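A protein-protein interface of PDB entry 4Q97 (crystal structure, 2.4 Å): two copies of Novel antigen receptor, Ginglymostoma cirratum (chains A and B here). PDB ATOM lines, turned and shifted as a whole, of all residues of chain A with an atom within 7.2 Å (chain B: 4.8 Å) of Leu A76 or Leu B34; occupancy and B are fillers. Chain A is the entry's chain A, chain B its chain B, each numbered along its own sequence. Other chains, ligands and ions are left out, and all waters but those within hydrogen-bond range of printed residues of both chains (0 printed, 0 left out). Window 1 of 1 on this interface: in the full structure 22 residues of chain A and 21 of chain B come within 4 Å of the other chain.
Hydrophobic or aromatic side chains of chain A that line the printed part of chain B: Val A32, Ala A59 and Leu A76.
Printed residues of chain B that touch a printed residue of chain A: Ser B14, Leu B34, Val B64 and Ser B72.
Along chain B the printed residues that touch a printed residue of chain A span positions 14 to 72.
Among the printed residues, no Asp or Glu carboxylate lies within 4 Å of a Lys or Arg side-chain nitrogen of the other chain.
Positions printed for both chains: 32, 33 and 74.
Of the 9 pairs that touch across the chains among the printed residues, none has its exchanged pair printed and touching as well.
The backbone carbonyl oxygen (O) of Ser A18 sits at hydrogen-bond distance from the side-chain amide nitrogen (NE2) of Gln A23, at 2.6 Å.
The backbone carbonyl oxygen (O) of Gln A30 is in hydrogen-bond range of the backbone NH (N) of Ser A18, at 2.9 Å.
N of Gln A30 sits close to NE2 of Gln A23 (3.4 Å).
N of Leu A76 is in hydrogen-bond range of O of Ala A59, 2.5 Å away.
OG1 of Thr A60 is in hydrogen-bond range of OG of Ser A75 (2.9 Å).
The backbone NH (N) of Leu B34 is in hydrogen-bond range of the backbone carbonyl oxygen (O) of Ser B14 (2.7 Å).
Printed residues of chain B within 4 Å of Gln A30: Leu B34 (3.4 Å).
Of the printed residues of chain B, Val A32 touches Leu B34.
Of the printed residues of chain B, Thr A60 touches Val B64.
Leu A77 touches none of the printed residues of chain B.
The nearest residue of chain B that does not touch Leu A76 is Val B64 (4.7 Å).
The nearest residue of chain A that does not touch Leu B34 is Ser A18 (4.9 Å).
The nearest printed residue of chain A that does not touch Ser B14 is Gln A30 (6.4 Å).
OG of Ser B14 lies close to OG of Ser A18, 3.2 Å away.
Among the printed residues, pairs that only touch across the chains: Gln A30 with Leu B34 (3.4 Å), Leu A76 with Leu B34 (3.4 Å), Thr A60 with Val B64 (3.5 Å), Leu A76 with Ser B72 (3.7 Å), Val A32 with Leu B34 (3.7 Å), Ala A59 with Val B64 (3.8 Å), Thr A61 with Val B64 (3.8 Å) and Gln A23 with Ser B14 (3.99 Å).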
ATOM      1  N   SER A  18      -2.830  23.167  22.663  1.00  0.00           N
ATOM      2  CA  SER A  18      -2.857  24.623  22.728  1.00  0.00           C
ATOM      3  C   SER A  18      -2.035  25.100  23.915  1.00  0.00           C
ATOM      4  O   SER A  18      -2.133  24.552  25.019  1.00  0.00           O
ATOM      5  CB  SER A  18      -4.286  25.164  22.810  1.00  0.00           C
ATOM      6  OG  SER A  18      -4.944  24.705  23.979  1.00  0.00           O
ATOM      7  N   GLN A  23      -3.101  29.690  29.748  1.00  0.00           N
ATOM      8  CA  GLN A  23      -2.533  28.351  29.818  1.00  0.00           C
ATOM      9  C   GLN A  23      -1.067  28.403  30.237  1.00  0.00           C
ATOM     10  O   GLN A  23      -0.697  27.816  31.258  1.00  0.00           O
ATOM     11  CB  GLN A  23      -2.709  27.625  28.484  1.00  0.00           C
ATOM     12  CG  GLN A  23      -4.166  27.331  28.150  1.00  0.00           C
ATOM     13  CD  GLN A  23      -4.347  26.740  26.770  1.00  0.00           C
ATOM     14  OE1 GLN A  23      -4.880  27.388  25.873  1.00  0.00           O
ATOM     15  NE2 GLN A  23      -3.901  25.505  26.591  1.00  0.00           N
ATOM     16  N   GLN A  30      -2.702  22.416  27.451  1.00  0.00           N
ATOM     17  CA  GLN A  30      -3.921  21.655  27.190  1.00  0.00           C
ATOM     18  C   GLN A  30      -3.782  20.810  25.931  1.00  0.00           C
ATOM     19  O   GLN A  30      -3.444  21.316  24.852  1.00  0.00           O
ATOM     20  CB  GLN A  30      -5.134  22.590  27.082  1.00  0.00           C
ATOM     21  CG  GLN A  30      -6.491  21.894  27.082  1.00  0.00           C
ATOM     22  CD  GLN A  30      -7.074  21.699  28.471  1.00  0.00           C
ATOM     23  OE1 GLN A  30      -6.371  21.833  29.484  1.00  0.00           O
ATOM     24  NE2 GLN A  30      -8.370  21.384  28.519  1.00  0.00           N
ATOM     25  N   LEU A  31      -4.029  19.515  26.096  1.00  0.00           N
ATOM     26  CA  LEU A  31      -4.056  18.578  24.985  1.00  0.00           C
ATOM     27  C   LEU A  31      -5.470  18.063  24.807  1.00  0.00           C
ATOM     28  O   LEU A  31      -6.154  17.760  25.783  1.00  0.00           O
ATOM     29  CB  LEU A  31      -3.102  17.408  25.220  1.00  0.00           C
ATOM     30  CG  LEU A  31      -1.615  17.695  25.410  1.00  0.00           C
ATOM     31  CD1 LEU A  31      -0.843  16.388  25.393  1.00  0.00           C
ATOM     32  CD2 LEU A  31      -1.078  18.635  24.343  1.00  0.00           C
ATOM     33  N   VAL A  32      -5.903  17.980  23.554  1.00  0.00           N
ATOM     34  CA  VAL A  32      -7.224  17.473  23.231  1.00  0.00           C
ATOM     35  C   VAL A  32      -7.086  16.219  22.376  1.00  0.00           C
ATOM     36  O   VAL A  32      -6.516  16.255  21.281  1.00  0.00           O
ATOM     37  CB  VAL A  32      -8.086  18.523  22.490  1.00  0.00           C
ATOM     38  CG1 VAL A  32      -9.444  17.942  22.115  1.00  0.00           C
ATOM     39  CG2 VAL A  32      -8.269  19.770  23.341  1.00  0.00           C
ATOM     40  N   CYS A  33      -7.601  15.109  22.888  1.00  0.00           N
ATOM     41  CA  CYS A  33      -7.742  13.918  22.066  1.00  0.00           C
ATOM     42  C   CYS A  33      -9.151  13.895  21.476  1.00  0.00           C
ATOM     43  O   CYS A  33     -10.110  13.485  22.131  1.00  0.00           O
ATOM     44  CB  CYS A  33      -7.440  12.654  22.872  1.00  0.00           C
ATOM     45  SG  CYS A  33      -7.472  11.128  21.911  1.00  0.00           S
ATOM     46  N   VAL A  45     -10.696   5.049  26.083  1.00  0.00           N
ATOM     47  CA  VAL A  45      -9.663   6.078  25.921  1.00  0.00           C
ATOM     48  C   VAL A  45      -8.606   5.947  27.010  1.00  0.00           C
ATOM     49  O   VAL A  45      -8.933   5.784  28.187  1.00  0.00           O
ATOM     50  CB  VAL A  45     -10.238   7.516  25.981  1.00  0.00           C
ATOM     51  CG1 VAL A  45      -9.211   8.530  25.488  1.00  0.00           C
ATOM     52  CG2 VAL A  45     -11.518   7.628  25.173  1.00  0.00           C
ATOM     53  N   TRP A  47      -4.466   7.562  28.026  1.00  0.00           N
ATOM     54  CA  TRP A  47      -3.358   8.464  27.767  1.00  0.00           C
ATOM     55  C   TRP A  47      -2.043   7.855  28.203  1.00  0.00           C
ATOM     56  O   TRP A  47      -1.993   7.113  29.188  1.00  0.00           O
ATOM     57  CB  TRP A  47      -3.557   9.757  28.546  1.00  0.00           C
ATOM     58  CG  TRP A  47      -4.635  10.629  28.021  1.00  0.00           C
ATOM     59  CD1 TRP A  47      -5.953  10.602  28.372  1.00  0.00           C
ATOM     60  CD2 TRP A  47      -4.493  11.676  27.055  1.00  0.00           C
ATOM     61  NE1 TRP A  47      -6.644  11.571  27.681  1.00  0.00           N
ATOM     62  CE2 TRP A  47      -5.771  12.244  26.866  1.00  0.00           C
ATOM     63  CE3 TRP A  47      -3.410  12.189  26.329  1.00  0.00           C
ATOM     64  CZ2 TRP A  47      -6.000  13.307  25.979  1.00  0.00           C
ATOM     65  CZ3 TRP A  47      -3.639  13.248  25.447  1.00  0.00           C
ATOM     66  CH2 TRP A  47      -4.925  13.793  25.282  1.00  0.00           C
ATOM     67  N   GLY A  57      -5.431  13.597  35.736  1.00  0.00           N
ATOM     68  CA  GLY A  57      -5.280  14.905  35.108  1.00  0.00           C
ATOM     69  C   GLY A  57      -6.081  15.018  33.822  1.00  0.00           C
ATOM     70  O   GLY A  57      -5.962  16.011  33.096  1.00  0.00           O
ATOM     71  N   PHE A  58      -6.901  14.005  33.535  1.00  0.00           N
ATOM     72  CA  PHE A  58      -7.692  14.008  32.308  1.00  0.00           C
ATOM     73  C   PHE A  58      -9.185  13.750  32.483  1.00  0.00           C
ATOM     74  O   PHE A  58      -9.605  12.898  33.272  1.00  0.00           O
ATOM     75  CB  PHE A  58      -7.082  13.091  31.234  1.00  0.00           C
ATOM     76  CG  PHE A  58      -7.208  11.620  31.518  1.00  0.00           C
ATOM     77  CD1 PHE A  58      -8.312  10.901  31.066  1.00  0.00           C
ATOM     78  CD2 PHE A  58      -6.200  10.937  32.195  1.00  0.00           C
ATOM     79  CE1 PHE A  58      -8.423   9.538  31.311  1.00  0.00           C
ATOM     80  CE2 PHE A  58      -6.305   9.573  32.441  1.00  0.00           C
ATOM     81  CZ  PHE A  58      -7.416   8.872  31.996  1.00  0.00           C
ATOM     82  N   ALA A  59      -9.972  14.517  31.733  1.00  0.00           N
ATOM     83  CA  ALA A  59     -11.411  14.332  31.649  1.00  0.00           C
ATOM     84  C   ALA A  59     -11.791  14.029  30.208  1.00  0.00           C
ATOM     85  O   ALA A  59     -11.176  14.541  29.268  1.00  0.00           O
ATOM     86  CB  ALA A  59     -12.136  15.575  32.140  1.00  0.00           C
ATOM     87  N   THR A  60     -12.796  13.180  30.041  1.00  0.00           N
ATOM     88  CA  THR A  60     -13.343  12.883  28.729  1.00  0.00           C
ATOM     89  C   THR A  60     -14.792  13.343  28.748  1.00  0.00           C
ATOM     90  O   THR A  60     -15.534  13.011  29.678  1.00  0.00           O
ATOM     91  CB  THR A  60     -13.234  11.377  28.397  1.00  0.00           C
ATOM     92  OG1 THR A  60     -11.859  10.969  28.462  1.00  0.00           O
ATOM     93  CG2 THR A  60     -13.774  11.077  26.998  1.00  0.00           C
ATOM     94  N   THR A  61     -15.180  14.126  27.741  1.00  0.00           N
ATOM     95  CA  THR A  61     -16.549  14.626  27.634  1.00  0.00           C
ATOM     96  C   THR A  61     -17.504  13.479  27.311  1.00  0.00           C
ATOM     97  O   THR A  61     -17.079  12.426  26.824  1.00  0.00           O
ATOM     98  CB  THR A  61     -16.695  15.733  26.556  1.00  0.00           C
ATOM     99  OG1 THR A  61     -16.552  15.171  25.244  1.00  0.00           O
ATOM    100  CG2 THR A  61     -15.662  16.853  26.755  1.00  0.00           C
ATOM    101  N   ALA A  74     -14.457  14.411  23.172  1.00  0.00           N
ATOM    102  CA  ALA A  74     -13.102  14.902  23.372  1.00  0.00           C
ATOM    103  C   ALA A  74     -12.576  14.421  24.715  1.00  0.00           C
ATOM    104  O   ALA A  74     -13.309  14.402  25.712  1.00  0.00           O
ATOM    105  CB  ALA A  74     -13.068  16.421  23.291  1.00  0.00           C
ATOM    106  N   SER A  75     -11.312  14.006  24.729  1.00  0.00           N
ATOM    107  CA  SER A  75     -10.624  13.696  25.974  1.00  0.00           C
ATOM    108  C   SER A  75      -9.607  14.791  26.265  1.00  0.00           C
ATOM    109  O   SER A  75      -8.719  15.065  25.449  1.00  0.00           O
ATOM    110  CB  SER A  75      -9.949  12.326  25.916  1.00  0.00           C
ATOM    111  OG  SER A  75      -9.466  11.960  27.198  1.00  0.00           O
ATOM    112  N   LEU A  76      -9.745  15.408  27.434  1.00  0.00           N
ATOM    113  CA  LEU A  76      -8.988  16.604  27.786  1.00  0.00           C
ATOM    114  C   LEU A  76      -7.935  16.352  28.858  1.00  0.00           C
ATOM    115  O   LEU A  76      -8.264  15.959  29.977  1.00  0.00           O
ATOM    116  CB  LEU A  76      -9.948  17.692  28.264  1.00  0.00           C
ATOM    117  CG  LEU A  76     -10.754  18.385  27.172  1.00  0.00           C
ATOM    118  CD1 LEU A  76     -12.024  19.007  27.731  1.00  0.00           C
ATOM    119  CD2 LEU A  76      -9.870  19.426  26.508  1.00  0.00           C
ATOM    120  N   LEU A  77      -6.675  16.592  28.506  1.00  0.00           N
ATOM    121  CA  LEU A  77      -5.574  16.450  29.446  1.00  0.00           C
ATOM    122  C   LEU A  77      -4.837  17.770  29.635  1.00  0.00           C
ATOM    123  O   LEU A  77      -4.417  18.409  28.661  1.00  0.00           O
ATOM    124  CB  LEU A  77      -4.606  15.349  28.999  1.00  0.00           C
ATOM    125  CG  LEU A  77      -3.284  15.185  29.767  1.00  0.00           C
ATOM    126  CD1 LEU A  77      -3.497  14.589  31.151  1.00  0.00           C
ATOM    127  CD2 LEU A  77      -2.302  14.336  28.977  1.00  0.00           C
ATOM    128  N   LYS A  78      -4.703  18.178  30.897  1.00  0.00           N
ATOM    129  CA  LYS A  78      -3.843  19.298  31.258  1.00  0.00           C
ATOM    130  C   LYS A  78      -2.495  18.716  31.630  1.00  0.00           C
ATOM    131  O   LYS A  78      -2.399  17.914  32.566  1.00  0.00           O
ATOM    132  CB  LYS A  78      -4.395  20.071  32.456  1.00  0.00           C
ATOM    133  CG  LYS A  78      -5.908  20.136  32.555  1.00  0.00           C
ATOM    134  CD  LYS A  78      -6.314  20.859  33.827  1.00  0.00           C
ATOM    135  CE  LYS A  78      -7.523  20.211  34.485  1.00  0.00           C
ATOM    136  NZ  LYS A  78      -7.570  20.512  35.947  1.00  0.00           N
ATOM    137  N   ILE B  12     -11.251  29.873  29.456  1.00  0.00           N
ATOM    138  CA  ILE B  12     -10.097  29.947  28.576  1.00  0.00           C
ATOM    139  C   ILE B  12     -10.559  29.353  27.256  1.00  0.00           C
ATOM    140  O   ILE B  12     -11.136  28.264  27.222  1.00  0.00           O
ATOM    141  CB  ILE B  12      -8.874  29.209  29.153  1.00  0.00           C
ATOM    142  CG1 ILE B  12      -8.542  29.759  30.551  1.00  0.00           C
ATOM    143  CG2 ILE B  12      -7.678  29.333  28.214  1.00  0.00           C
ATOM    144  CD1 ILE B  12      -7.483  28.964  31.301  1.00  0.00           C
ATOM    145  N   VAL B  13     -10.333  30.101  26.181  1.00  0.00           N
ATOM    146  CA  VAL B  13     -10.881  29.783  24.869  1.00  0.00           C
ATOM    147  C   VAL B  13      -9.752  29.519  23.896  1.00  0.00           C
ATOM    148  O   VAL B  13      -8.819  30.313  23.773  1.00  0.00           O
ATOM    149  CB  VAL B  13     -11.749  30.941  24.341  1.00  0.00           C
ATOM    150  CG1 VAL B  13     -12.151  30.713  22.888  1.00  0.00           C
ATOM    151  CG2 VAL B  13     -12.971  31.100  25.225  1.00  0.00           C
ATOM    152  N   SER B  14      -9.832  28.394  23.206  1.00  0.00           N
ATOM    153  CA  SER B  14      -8.792  28.067  22.264  1.00  0.00           C
ATOM    154  C   SER B  14      -9.376  27.306  21.080  1.00  0.00           C
ATOM    155  O   SER B  14     -10.093  26.311  21.246  1.00  0.00           O
ATOM    156  CB  SER B  14      -7.637  27.357  22.984  1.00  0.00           C
ATOM    157  OG  SER B  14      -7.126  26.262  22.253  1.00  0.00           O
ATOM    158  N   VAL B  32     -12.050  22.693  16.547  1.00  0.00           N
ATOM    159  CA  VAL B  32     -12.455  22.523  17.931  1.00  0.00           C
ATOM    160  C   VAL B  32     -12.371  23.863  18.648  1.00  0.00           C
ATOM    161  O   VAL B  32     -11.303  24.470  18.734  1.00  0.00           O
ATOM    162  CB  VAL B  32     -11.581  21.476  18.668  1.00  0.00           C
ATOM    163  CG1 VAL B  32     -11.993  21.361  20.131  1.00  0.00           C
ATOM    164  CG2 VAL B  32     -11.677  20.119  17.992  1.00  0.00           C
ATOM    165  N   CYS B  33     -13.506  24.331  19.149  1.00  0.00           N
ATOM    166  CA  CYS B  33     -13.503  25.464  20.060  1.00  0.00           C
ATOM    167  C   CYS B  33     -13.473  24.942  21.494  1.00  0.00           C
ATOM    168  O   CYS B  33     -14.503  24.569  22.051  1.00  0.00           O
ATOM    169  CB  CYS B  33     -14.712  26.364  19.812  1.00  0.00           C
ATOM    170  SG  CYS B  33     -14.761  27.878  20.795  1.00  0.00           S
ATOM    171  N   LEU B  34     -12.273  24.896  22.072  1.00  0.00           N
ATOM    172  CA  LEU B  34     -12.097  24.471  23.452  1.00  0.00           C
ATOM    173  C   LEU B  34     -12.343  25.597  24.430  1.00  0.00           C
ATOM    174  O   LEU B  34     -11.705  26.650  24.356  1.00  0.00           O
ATOM    175  CB  LEU B  34     -10.696  23.924  23.686  1.00  0.00           C
ATOM    176  CG  LEU B  34     -10.650  23.129  24.982  1.00  0.00           C
ATOM    177  CD1 LEU B  34     -11.512  21.878  24.853  1.00  0.00           C
ATOM    178  CD2 LEU B  34      -9.217  22.784  25.297  1.00  0.00           C
ATOM    179  N   ILE B  35     -13.260  25.341  25.360  1.00  0.00           N
ATOM    180  CA  ILE B  35     -13.675  26.294  26.379  1.00  0.00           C
ATOM    181  C   ILE B  35     -13.512  25.643  27.752  1.00  0.00           C
ATOM    182  O   ILE B  35     -14.311  24.781  28.133  1.00  0.00           O
ATOM    183  CB  ILE B  35     -15.161  26.665  26.216  1.00  0.00           C
ATOM    184  CG1 ILE B  35     -15.493  27.005  24.758  1.00  0.00           C
ATOM    185  CG2 ILE B  35     -15.523  27.804  27.160  1.00  0.00           C
ATOM    186  CD1 ILE B  35     -16.977  26.946  24.431  1.00  0.00           C
ATOM    187  N   SER B  36     -12.494  26.066  28.497  1.00  0.00           N
ATOM    188  CA  SER B  36     -12.139  25.416  29.759  1.00  0.00           C
ATOM    189  C   SER B  36     -11.861  26.416  30.871  1.00  0.00           C
ATOM    190  O   SER B  36     -11.389  27.520  30.617  1.00  0.00           O
ATOM    191  CB  SER B  36     -10.897  24.547  29.552  1.00  0.00           C
ATOM    192  OG  SER B  36      -9.841  25.331  29.045  1.00  0.00           O
ATOM    193  N   VAL B  64     -17.683  18.942  31.271  1.00  0.00           N
ATOM    194  CA  VAL B  64     -17.181  18.119  32.363  1.00  0.00           C
ATOM    195  C   VAL B  64     -16.582  18.980  33.463  1.00  0.00           C
ATOM    196  O   VAL B  64     -16.091  20.089  33.221  1.00  0.00           O
ATOM    197  CB  VAL B  64     -16.128  17.084  31.909  1.00  0.00           C
ATOM    198  CG1 VAL B  64     -16.796  15.934  31.177  1.00  0.00           C
ATOM    199  CG2 VAL B  64     -15.044  17.735  31.056  1.00  0.00           C
ATOM    200  N   SER B  72     -14.972  22.269  31.638  1.00  0.00           N
ATOM    201  CA  SER B  72     -14.460  22.319  30.280  1.00  0.00           C
ATOM    202  C   SER B  72     -15.505  21.733  29.345  1.00  0.00           C
ATOM    203  O   SER B  72     -16.233  20.811  29.713  1.00  0.00           O
ATOM    204  CB  SER B  72     -13.158  21.534  30.159  1.00  0.00           C
ATOM    205  OG  SER B  72     -12.138  22.099  30.963  1.00  0.00           O
ATOM    206  N   CYS B  73     -15.593  22.286  28.144  1.00  0.00           N
ATOM    207  CA  CYS B  73     -16.400  21.678  27.099  1.00  0.00           C
ATOM    208  C   CYS B  73     -15.767  21.992  25.760  1.00  0.00           C
ATOM    209  O   CYS B  73     -14.877  22.840  25.674  1.00  0.00           O
ATOM    210  CB  CYS B  73     -17.861  22.146  27.165  1.00  0.00           C
ATOM    211  SG  CYS B  73     -18.200  23.788  26.493  1.00  0.00           S
ATOM    212  N   ALA B  74     -16.204  21.285  24.725  1.00  0.00           N
ATOM    213  CA  ALA B  74     -15.693  21.519  23.383  1.00  0.00           C
ATOM    214  C   ALA B  74     -16.854  21.754  22.433  1.00  0.00           C
ATOM    215  O   ALA B  74     -17.887  21.077  22.523  1.00  0.00           O
ATOM    216  CB  ALA B  74     -14.849  20.341  22.921  1.00  0.00           C
